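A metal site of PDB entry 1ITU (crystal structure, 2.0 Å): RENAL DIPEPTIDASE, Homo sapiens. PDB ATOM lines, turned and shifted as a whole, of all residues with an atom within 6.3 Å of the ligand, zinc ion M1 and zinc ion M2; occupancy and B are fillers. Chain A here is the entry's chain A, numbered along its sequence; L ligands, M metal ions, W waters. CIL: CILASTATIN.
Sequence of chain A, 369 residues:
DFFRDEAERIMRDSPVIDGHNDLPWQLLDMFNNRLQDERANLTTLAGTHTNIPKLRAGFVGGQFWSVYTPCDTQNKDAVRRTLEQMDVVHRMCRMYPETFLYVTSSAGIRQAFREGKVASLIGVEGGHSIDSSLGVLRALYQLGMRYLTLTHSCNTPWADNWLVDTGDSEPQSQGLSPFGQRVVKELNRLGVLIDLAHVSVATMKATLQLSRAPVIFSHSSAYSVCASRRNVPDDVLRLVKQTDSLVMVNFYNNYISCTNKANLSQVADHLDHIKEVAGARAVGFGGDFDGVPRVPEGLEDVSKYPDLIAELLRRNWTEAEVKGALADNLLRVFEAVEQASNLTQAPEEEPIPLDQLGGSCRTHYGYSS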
ATOM      1  N   HIS A  20       8.457 -30.132  20.888  1.00  0.00           N
ATOM      2  CA  HIS A  20       7.518 -30.785  21.795  1.00  0.00           C
ATOM      3  C   HIS A  20       6.127 -31.075  21.241  1.00  0.00           C
ATOM      4  O   HIS A  20       5.314 -30.180  21.089  1.00  0.00           O
ATOM      5  CB  HIS A  20       7.370 -29.969  23.065  1.00  0.00           C
ATOM      6  CG  HIS A  20       6.763 -30.724  24.201  1.00  0.00           C
ATOM      7  ND1 HIS A  20       7.495 -31.515  25.071  1.00  0.00           N
ATOM      8  CD2 HIS A  20       5.473 -30.819  24.610  1.00  0.00           C
ATOM      9  CE1 HIS A  20       6.648 -32.036  25.959  1.00  0.00           C
ATOM     10  NE2 HIS A  20       5.411 -31.643  25.726  1.00  0.00           N
ATOM     11  N   ASN A  21       5.838 -32.355  21.024  1.00  0.00           N
ATOM     12  CA  ASN A  21       4.539 -32.764  20.537  1.00  0.00           C
ATOM     13  C   ASN A  21       4.036 -33.933  21.400  1.00  0.00           C
ATOM     14  O   ASN A  21       4.733 -34.944  21.544  1.00  0.00           O
ATOM     15  CB  ASN A  21       4.647 -33.177  19.072  1.00  0.00           C
ATOM     16  CG  ASN A  21       3.317 -33.561  18.481  1.00  0.00           C
ATOM     17  OD1 ASN A  21       2.655 -34.477  18.960  1.00  0.00           O
ATOM     18  ND2 ASN A  21       2.918 -32.858  17.431  1.00  0.00           N
ATOM     19  N   ASP A  22       2.866 -33.769  22.005  1.00  0.00           N
ATOM     20  CA  ASP A  22       2.279 -34.792  22.871  1.00  0.00           C
ATOM     21  C   ASP A  22       1.399 -35.858  22.210  1.00  0.00           C
ATOM     22  O   ASP A  22       0.445 -36.341  22.833  1.00  0.00           O
ATOM     23  CB  ASP A  22       1.492 -34.145  24.014  1.00  0.00           C
ATOM     24  CG  ASP A  22       2.379 -33.724  25.167  1.00  0.00           C
ATOM     25  OD1 ASP A  22       2.301 -32.550  25.553  1.00  0.00           O
ATOM     26  OD2 ASP A  22       3.122 -34.578  25.706  1.00  0.00           O
ATOM     27  N   TRP A  25       0.895 -39.207  24.198  1.00  0.00           N
ATOM     28  CA  TRP A  25      -0.082 -39.110  25.284  1.00  0.00           C
ATOM     29  C   TRP A  25      -1.491 -39.374  24.749  1.00  0.00           C
ATOM     30  O   TRP A  25      -2.324 -39.975  25.427  1.00  0.00           O
ATOM     31  CB  TRP A  25      -0.016 -37.714  25.896  1.00  0.00           C
ATOM     32  CG  TRP A  25      -1.150 -37.408  26.792  1.00  0.00           C
ATOM     33  CD1 TRP A  25      -2.148 -36.509  26.573  1.00  0.00           C
ATOM     34  CD2 TRP A  25      -1.444 -38.043  28.042  1.00  0.00           C
ATOM     35  NE1 TRP A  25      -3.045 -36.532  27.603  1.00  0.00           N
ATOM     36  CE2 TRP A  25      -2.638 -37.463  28.520  1.00  0.00           C
ATOM     37  CE3 TRP A  25      -0.812 -39.031  28.794  1.00  0.00           C
ATOM     38  CZ2 TRP A  25      -3.220 -37.849  29.740  1.00  0.00           C
ATOM     39  CZ3 TRP A  25      -1.392 -39.427  30.004  1.00  0.00           C
ATOM     40  CH2 TRP A  25      -2.580 -38.833  30.457  1.00  0.00           C
ATOM     41  N   GLN A  26      -1.754 -38.870  23.544  1.00  0.00           N
ATOM     42  CA  GLN A  26      -3.037 -39.058  22.879  1.00  0.00           C
ATOM     43  C   GLN A  26      -3.219 -40.529  22.477  1.00  0.00           C
ATOM     44  O   GLN A  26      -4.304 -41.072  22.575  1.00  0.00           O
ATOM     45  CB  GLN A  26      -3.109 -38.163  21.648  1.00  0.00           C
ATOM     46  CG  GLN A  26      -3.066 -36.669  21.967  1.00  0.00           C
ATOM     47  CD  GLN A  26      -4.258 -36.221  22.781  1.00  0.00           C
ATOM     48  OE1 GLN A  26      -5.356 -36.759  22.640  1.00  0.00           O
ATOM     49  NE2 GLN A  26      -4.047 -35.232  23.650  1.00  0.00           N
ATOM     50  N   SER A  66       7.068 -36.120  22.763  1.00  0.00           N
ATOM     51  CA  SER A  66       7.011 -36.101  24.209  1.00  0.00           C
ATOM     52  C   SER A  66       6.583 -37.425  24.834  1.00  0.00           C
ATOM     53  O   SER A  66       5.589 -38.044  24.416  1.00  0.00           O
ATOM     54  CB  SER A  66       6.066 -34.992  24.678  1.00  0.00           C
ATOM     55  OG  SER A  66       5.893 -35.047  26.081  1.00  0.00           O
ATOM     56  N   TYR A  68       5.440 -38.292  28.100  1.00  0.00           N
ATOM     57  CA  TYR A  68       4.902 -37.657  29.276  1.00  0.00           C
ATOM     58  C   TYR A  68       3.995 -38.560  30.106  1.00  0.00           C
ATOM     59  O   TYR A  68       3.160 -39.285  29.566  1.00  0.00           O
ATOM     60  CB  TYR A  68       4.152 -36.399  28.825  1.00  0.00           C
ATOM     61  CG  TYR A  68       3.110 -35.912  29.778  1.00  0.00           C
ATOM     62  CD1 TYR A  68       1.761 -36.183  29.555  1.00  0.00           C
ATOM     63  CD2 TYR A  68       3.456 -35.172  30.908  1.00  0.00           C
ATOM     64  CE1 TYR A  68       0.776 -35.739  30.444  1.00  0.00           C
ATOM     65  CE2 TYR A  68       2.488 -34.724  31.798  1.00  0.00           C
ATOM     66  CZ  TYR A  68       1.149 -35.006  31.559  1.00  0.00           C
ATOM     67  OH  TYR A  68       0.190 -34.572  32.447  1.00  0.00           O
ATOM     68  N   GLU A 125       9.212 -35.616  29.412  1.00  0.00           N
ATOM     69  CA  GLU A 125       8.608 -34.476  30.095  1.00  0.00           C
ATOM     70  C   GLU A 125       8.320 -34.591  31.580  1.00  0.00           C
ATOM     71  O   GLU A 125       7.191 -34.854  31.993  1.00  0.00           O
ATOM     72  CB  GLU A 125       7.358 -34.004  29.342  1.00  0.00           C
ATOM     73  CG  GLU A 125       6.874 -32.672  29.882  1.00  0.00           C
ATOM     74  CD  GLU A 125       5.696 -32.064  29.175  1.00  0.00           C
ATOM     75  OE1 GLU A 125       4.893 -32.783  28.551  1.00  0.00           O
ATOM     76  OE2 GLU A 125       5.563 -30.835  29.272  1.00  0.00           O
ATOM     77  N   HIS A 152       7.544 -31.253  35.451  1.00  0.00           N
ATOM     78  CA  HIS A 152       6.376 -31.004  34.651  1.00  0.00           C
ATOM     79  C   HIS A 152       5.705 -29.967  35.568  1.00  0.00           C
ATOM     80  O   HIS A 152       6.390 -29.083  36.074  1.00  0.00           O
ATOM     81  CB  HIS A 152       5.474 -32.231  34.447  1.00  0.00           C
ATOM     82  CG  HIS A 152       4.296 -31.930  33.583  1.00  0.00           C
ATOM     83  ND1 HIS A 152       3.003 -31.907  34.066  1.00  0.00           N
ATOM     84  CD2 HIS A 152       4.212 -31.505  32.299  1.00  0.00           C
ATOM     85  CE1 HIS A 152       2.183 -31.472  33.120  1.00  0.00           C
ATOM     86  NE2 HIS A 152       2.895 -31.228  32.038  1.00  0.00           N
ATOM     87  N   SER A 153       4.410 -30.102  35.824  1.00  0.00           N
ATOM     88  CA  SER A 153       3.716 -29.155  36.693  1.00  0.00           C
ATOM     89  C   SER A 153       3.607 -29.615  38.148  1.00  0.00           C
ATOM     90  O   SER A 153       2.553 -29.507  38.791  1.00  0.00           O
ATOM     91  CB  SER A 153       2.362 -28.779  36.111  1.00  0.00           C
ATOM     92  OG  SER A 153       2.552 -28.175  34.849  1.00  0.00           O
ATOM     93  N   TRP A 162       7.156 -24.574  37.731  1.00  0.00           N
ATOM     94  CA  TRP A 162       6.651 -23.238  37.461  1.00  0.00           C
ATOM     95  C   TRP A 162       5.546 -22.754  38.395  1.00  0.00           C
ATOM     96  O   TRP A 162       5.397 -21.552  38.594  1.00  0.00           O
ATOM     97  CB  TRP A 162       6.205 -23.122  36.008  1.00  0.00           C
ATOM     98  CG  TRP A 162       4.896 -23.773  35.725  1.00  0.00           C
ATOM     99  CD1 TRP A 162       4.651 -25.117  35.562  1.00  0.00           C
ATOM    100  CD2 TRP A 162       3.632 -23.114  35.544  1.00  0.00           C
ATOM    101  NE1 TRP A 162       3.324 -25.329  35.280  1.00  0.00           N
ATOM    102  CE2 TRP A 162       2.673 -24.121  35.258  1.00  0.00           C
ATOM    103  CE3 TRP A 162       3.220 -21.778  35.590  1.00  0.00           C
ATOM    104  CZ2 TRP A 162       1.332 -23.813  35.009  1.00  0.00           C
ATOM    105  CZ3 TRP A 162       1.885 -21.474  35.347  1.00  0.00           C
ATOM    106  CH2 TRP A 162       0.959 -22.493  35.054  1.00  0.00           C
ATOM    107  N   ALA A 197      11.379 -26.108  30.216  1.00  0.00           N
ATOM    108  CA  ALA A 197       9.947 -25.865  30.129  1.00  0.00           C
ATOM    109  C   ALA A 197       9.372 -26.368  31.462  1.00  0.00           C
ATOM    110  O   ALA A 197       9.921 -27.290  32.079  1.00  0.00           O
ATOM    111  CB  ALA A 197       9.339 -26.665  28.965  1.00  0.00           C
ATOM    112  N   HIS A 198       8.328 -25.688  31.955  1.00  0.00           N
ATOM    113  CA  HIS A 198       7.648 -26.070  33.192  1.00  0.00           C
ATOM    114  C   HIS A 198       8.358 -25.870  34.521  1.00  0.00           C
ATOM    115  O   HIS A 198       7.805 -26.225  35.553  1.00  0.00           O
ATOM    116  CB  HIS A 198       7.200 -27.542  33.136  1.00  0.00           C
ATOM    117  CG  HIS A 198       6.040 -27.806  32.239  1.00  0.00           C
ATOM    118  ND1 HIS A 198       4.722 -27.710  32.641  1.00  0.00           N
ATOM    119  CD2 HIS A 198       6.006 -28.207  30.942  1.00  0.00           C
ATOM    120  CE1 HIS A 198       3.961 -28.053  31.598  1.00  0.00           C
ATOM    121  NE2 HIS A 198       4.688 -28.352  30.544  1.00  0.00           N
ATOM    122  N   HIS A 219       9.161 -26.033  24.922  1.00  0.00           N
ATOM    123  CA  HIS A 219       7.872 -25.444  24.603  1.00  0.00           C
ATOM    124  C   HIS A 219       7.460 -24.361  25.623  1.00  0.00           C
ATOM    125  O   HIS A 219       6.618 -24.572  26.503  1.00  0.00           O
ATOM    126  CB  HIS A 219       6.781 -26.536  24.401  1.00  0.00           C
ATOM    127  CG  HIS A 219       6.562 -27.428  25.574  1.00  0.00           C
ATOM    128  ND1 HIS A 219       7.558 -28.172  26.186  1.00  0.00           N
ATOM    129  CD2 HIS A 219       5.441 -27.674  26.286  1.00  0.00           C
ATOM    130  CE1 HIS A 219       7.022 -28.822  27.217  1.00  0.00           C
ATOM    131  NE2 HIS A 219       5.730 -28.548  27.317  1.00  0.00           N
ATOM    132  N   ARG A 230       4.550 -19.963  32.685  1.00  0.00           N
ATOM    133  CA  ARG A 230       5.016 -21.057  31.860  1.00  0.00           C
ATOM    134  C   ARG A 230       5.913 -20.439  30.792  1.00  0.00           C
ATOM    135  O   ARG A 230       6.551 -21.138  30.006  1.00  0.00           O
ATOM    136  CB  ARG A 230       3.846 -21.809  31.225  1.00  0.00           C
ATOM    137  CG  ARG A 230       3.427 -23.031  32.024  1.00  0.00           C
ATOM    138  CD  ARG A 230       4.501 -24.113  31.928  1.00  0.00           C
ATOM    139  NE  ARG A 230       4.420 -24.833  30.658  1.00  0.00           N
ATOM    140  CZ  ARG A 230       5.341 -24.816  29.707  1.00  0.00           C
ATOM    141  NH1 ARG A 230       5.163 -25.520  28.594  1.00  0.00           N
ATOM    142  NH2 ARG A 230       6.437 -24.078  29.852  1.00  0.00           N
ATOM    143  N   ASN A 250       6.035 -22.183  22.295  1.00  0.00           N
ATOM    144  CA  ASN A 250       4.798 -22.937  22.537  1.00  0.00           C
ATOM    145  C   ASN A 250       3.637 -22.200  21.864  1.00  0.00           C
ATOM    146  O   ASN A 250       3.540 -20.976  21.970  1.00  0.00           O
ATOM    147  CB  ASN A 250       4.595 -23.018  24.056  1.00  0.00           C
ATOM    148  CG  ASN A 250       3.479 -23.972  24.466  1.00  0.00           C
ATOM    149  OD1 ASN A 250       2.474 -24.117  23.782  1.00  0.00           O
ATOM    150  ND2 ASN A 250       3.650 -24.586  25.644  1.00  0.00           N
ATOM    151  N   TYR A 252       0.307 -22.694  22.528  1.00  0.00           N
ATOM    152  CA  TYR A 252      -0.895 -22.645  23.362  1.00  0.00           C
ATOM    153  C   TYR A 252      -1.428 -21.200  23.495  1.00  0.00           C
ATOM    154  O   TYR A 252      -0.695 -20.304  23.905  1.00  0.00           O
ATOM    155  CB  TYR A 252      -0.581 -23.224  24.757  1.00  0.00           C
ATOM    156  CG  TYR A 252      -1.759 -23.365  25.704  1.00  0.00           C
ATOM    157  CD1 TYR A 252      -1.580 -23.230  27.078  1.00  0.00           C
ATOM    158  CD2 TYR A 252      -3.031 -23.689  25.230  1.00  0.00           C
ATOM    159  CE1 TYR A 252      -2.628 -23.423  27.964  1.00  0.00           C
ATOM    160  CE2 TYR A 252      -4.103 -23.884  26.121  1.00  0.00           C
ATOM    161  CZ  TYR A 252      -3.889 -23.739  27.485  1.00  0.00           C
ATOM    162  OH  TYR A 252      -4.921 -23.928  28.373  1.00  0.00           O
ATOM    163  N   TYR A 255      -0.875 -19.073  26.587  1.00  0.00           N
ATOM    164  CA  TYR A 255       0.508 -18.705  26.853  1.00  0.00           C
ATOM    165  C   TYR A 255       0.957 -17.672  25.808  1.00  0.00           C
ATOM    166  O   TYR A 255       1.989 -17.016  25.946  1.00  0.00           O
ATOM    167  CB  TYR A 255       1.449 -19.927  26.794  1.00  0.00           C
ATOM    168  CG  TYR A 255       1.172 -20.989  27.842  1.00  0.00           C
ATOM    169  CD1 TYR A 255       0.314 -20.751  28.920  1.00  0.00           C
ATOM    170  CD2 TYR A 255       1.774 -22.248  27.742  1.00  0.00           C
ATOM    171  CE1 TYR A 255       0.049 -21.740  29.868  1.00  0.00           C
ATOM    172  CE2 TYR A 255       1.501 -23.255  28.687  1.00  0.00           C
ATOM    173  CZ  TYR A 255       0.647 -22.990  29.734  1.00  0.00           C
ATOM    174  OH  TYR A 255       0.372 -23.997  30.635  1.00  0.00           O
ATOM    175  N   ASP A 288       3.688 -27.555  21.114  1.00  0.00           N
ATOM    176  CA  ASP A 288       2.883 -28.206  22.152  1.00  0.00           C
ATOM    177  C   ASP A 288       1.589 -28.781  21.559  1.00  0.00           C
ATOM    178  O   ASP A 288       0.587 -28.941  22.260  1.00  0.00           O
ATOM    179  CB  ASP A 288       2.587 -27.223  23.303  1.00  0.00           C
ATOM    180  CG  ASP A 288       2.333 -27.914  24.630  1.00  0.00           C
ATOM    181  OD1 ASP A 288       2.478 -29.165  24.702  1.00  0.00           O
ATOM    182  OD2 ASP A 288       2.004 -27.222  25.605  1.00  0.00           O
ATOM    183  N   ASP A 290      -1.116 -31.344  20.365  1.00  0.00           N
ATOM    184  CA  ASP A 290      -1.605 -32.574  20.984  1.00  0.00           C
ATOM    185  C   ASP A 290      -1.360 -32.643  22.501  1.00  0.00           C
ATOM    186  O   ASP A 290      -1.631 -33.662  23.154  1.00  0.00           O
ATOM    187  CB  ASP A 290      -1.105 -33.814  20.248  1.00  0.00           C
ATOM    188  CG  ASP A 290      -1.957 -34.145  19.028  1.00  0.00           C
ATOM    189  OD1 ASP A 290      -3.204 -34.019  19.116  1.00  0.00           O
ATOM    190  OD2 ASP A 290      -1.393 -34.522  17.986  1.00  0.00           O
ATOM    191  N   GLY A 291      -0.908 -31.527  23.048  1.00  0.00           N
ATOM    192  CA  GLY A 291      -0.685 -31.421  24.469  1.00  0.00           C
ATOM    193  C   GLY A 291      -1.508 -30.282  25.024  1.00  0.00           C
ATOM    194  O   GLY A 291      -1.558 -30.080  26.233  1.00  0.00           O
ATOM    195  N   VAL A 292      -2.182 -29.536  24.148  1.00  0.00           N
ATOM    196  CA  VAL A 292      -2.999 -28.392  24.567  1.00  0.00           C
ATOM    197  C   VAL A 292      -4.401 -28.449  23.987  1.00  0.00           C
ATOM    198  O   VAL A 292      -4.634 -29.031  22.924  1.00  0.00           O
ATOM    199  CB  VAL A 292      -2.365 -27.047  24.152  1.00  0.00           C
ATOM    200  CG1 VAL A 292      -1.017 -26.902  24.789  1.00  0.00           C
ATOM    201  CG2 VAL A 292      -2.252 -26.964  22.643  1.00  0.00           C
ATOM    202  N   PRO A 293      -5.377 -27.821  24.683  1.00  0.00           N
ATOM    203  CA  PRO A 293      -6.769 -27.788  24.223  1.00  0.00           C
ATOM    204  C   PRO A 293      -7.082 -26.659  23.236  1.00  0.00           C
ATOM    205  O   PRO A 293      -8.108 -26.704  22.542  1.00  0.00           O
ATOM    206  CB  PRO A 293      -7.532 -27.577  25.539  1.00  0.00           C
ATOM    207  CG  PRO A 293      -6.615 -26.705  26.301  1.00  0.00           C
ATOM    208  CD  PRO A 293      -5.269 -27.359  26.068  1.00  0.00           C
ATOM    209  N   ARG A 294      -6.215 -25.647  23.177  1.00  0.00           N
ATOM    210  CA  ARG A 294      -6.432 -24.496  22.308  1.00  0.00           C
ATOM    211  C   ARG A 294      -5.189 -24.080  21.543  1.00  0.00           C
ATOM    212  O   ARG A 294      -4.147 -23.841  22.132  1.00  0.00           O
ATOM    213  CB  ARG A 294      -6.918 -23.283  23.134  1.00  0.00           C
ATOM    214  CG  ARG A 294      -8.366 -23.374  23.571  1.00  0.00           C
ATOM    215  CD  ARG A 294      -8.705 -22.338  24.615  1.00  0.00           C
ATOM    216  NE  ARG A 294      -7.978 -22.556  25.854  1.00  0.00           N
ATOM    217  CZ  ARG A 294      -8.387 -23.340  26.850  1.00  0.00           C
ATOM    218  NH1 ARG A 294      -7.660 -23.472  27.947  1.00  0.00           N
ATOM    219  NH2 ARG A 294      -9.541 -23.997  26.748  1.00  0.00           N
HETATM  220  C1  CIL L   1       1.206 -32.538  29.057  1.00  0.00           C
HETATM  221  C2  CIL L   1       0.564 -31.341  28.427  1.00  0.00           C
HETATM  222  C3  CIL L   1      -0.278 -32.321  29.179  1.00  0.00           C
HETATM  223  C4  CIL L   1      -0.826 -31.909  30.526  1.00  0.00           C
HETATM  224  C5  CIL L   1      -1.201 -33.207  28.385  1.00  0.00           C
HETATM  225  C6  CIL L   1       0.817 -30.023  28.982  1.00  0.00           C
HETATM  226  N7  CIL L   1       0.364 -28.936  28.246  1.00  0.00           N
HETATM  227  C8  CIL L   1       0.533 -27.645  28.640  1.00  0.00           C
HETATM  228  C9  CIL L   1      -0.517 -26.820  28.749  1.00  0.00           C
HETATM  229  O10 CIL L   1       1.412 -29.879  30.041  1.00  0.00           O
HETATM  230  C11 CIL L   1       1.919 -27.087  28.944  1.00  0.00           C
HETATM  231  O12 CIL L   1       2.063 -26.281  29.867  1.00  0.00           O
HETATM  232  O13 CIL L   1       2.873 -27.435  28.275  1.00  0.00           O
HETATM  233  C14 CIL L   1      -1.930 -27.222  28.490  1.00  0.00           C
HETATM  234  C15 CIL L   1      -2.703 -27.148  29.792  1.00  0.00           C
HETATM  235  C16 CIL L   1      -4.206 -27.231  29.512  1.00  0.00           C
HETATM  236 ZN    ZN M   1       4.215 -29.249  28.573  1.00  0.00          ZN
HETATM  237 ZN    ZN M   2       3.786 -32.027  26.860  1.00  0.00          ZN
HETATM  238  O   HOH W   1       2.906 -30.000  27.071  1.00  0.00           O
HETATM  239  O   HOH W   2      -1.675 -30.474  33.350  1.00  0.00           O
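A ring nitrogen (NE2) of His 152 is in hydrogen-bond range of an oxygen (O10) of the ligand (2.8 Å). NE of Arg 230 lies within salt-bridge range of O12 of the ligand, 2.9 Å away. An oxygen (O12) of the ligand lies within hydrogen-bond range of the side-chain hydroxyl (OH) of Tyr 255 (2.9 Å). A nitrogen (N7) of the ligand is in hydrogen-bond range of the backbone carbonyl oxygen (O) of Gly 291 (3.0 Å).
The backbone NH (N) of Asp 288 lies within hydrogen-bond range of the backbone carbonyl oxygen (O) of His 20, 3.1 Å away. The side-chain hydroxyl (OG) of Ser 66 is in hydrogen-bond range of the side-chain carboxylate (OD2) of Asp 22, at 2.8 Å. A ring nitrogen (NE2) of His 198 sits close to the guanidinium group (NH1) of Arg 230. The side-chain hydroxyl of Ser 153 lies within hydrogen-bond range of a ring nitrogen (ND1) of His 198, 3.1 Å away. N of Trp 162 sits at hydrogen-bond distance from O of His 198. OD1 of Asn 250 sits at hydrogen-bond distance from N of Tyr 252 (2.9 Å). OH of Tyr 252 is in hydrogen-bond range of NH1 of Arg 294 (2.8 Å). The backbone NH (N) of Ser 66 lies within hydrogen-bond range of the backbone carbonyl oxygen (O) of Asn 21, 2.9 Å away.
An oxygen (O13) of the ligand sits close to the side-chain carboxylate (OD2) of Asp 288. Residues that only touch the ligand: Trp 25 (3.9 Å), Tyr 68 (3.4 Å), Asn 250 (3.96 Å), Tyr 252 (3.6 Å), Val 292 (3.8 Å) and Pro 293 (3.6 Å). Hydrophobic or aromatic side chains within 4 Å of the ligand: Trp 25, Tyr 68, His 152, His 198, His 219, Tyr 252, Tyr 255, Val 292 and Pro 293. 15 residues have an atom within 4 Å of the ligand: Asp 22, Trp 25, Tyr 68, Glu 125, His 152, His 198, His 219, Arg 230, Asn 250, Tyr 252, Tyr 255, Asp 288, Gly 291, Val 292 and Pro 293. The nearest printed residue that does not touch the ligand is Ser 153 (5.2 Å).
Merely in contact with zinc ion M1: Arg 230. Of the 24 residues printed, 5 come within 4 Å of zinc ion M1. Along chain A the residues within 4 Å of zinc ion M1 span positions 20 to 230.
OG of Ser 66 touches zinc ion M2 (3.8 Å). Asp 288 touches zinc ion M2. Within 4 Å of zinc ion M2: His 20, Asp 22, Ser 66, Glu 125 and Asp 288.
NE2 of His 219 is bound to zinc ion M1 (2.1 Å). Water W1 is bound to zinc ion M1 (2.1 Å). The side-chain carboxylate (OE2) of Glu 125 is bound to zinc ion M1, at 2.2 Å. NE2 of His 198 binds zinc ion M1 (2.2 Å). Zinc ion M1 is bound by O13 of the ligand (2.3 Å). Zinc ion M1 has five donor atoms within binding distance.
NE2 of His 20 is bound to zinc ion M2, at 2.0 Å. OD1 of Asp 22 is bound to zinc ion M2 (2.0 Å). The side-chain carboxylate (OE1) of Glu 125 binds zinc ion M2. Water W1 is bound to zinc ion M2, at 2.2 Å.
Water W1 bridges the side-chain carboxylate (OD1) of Asp 288 (2.5 Å) and a nitrogen (N7) of the ligand (3.0 Å).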
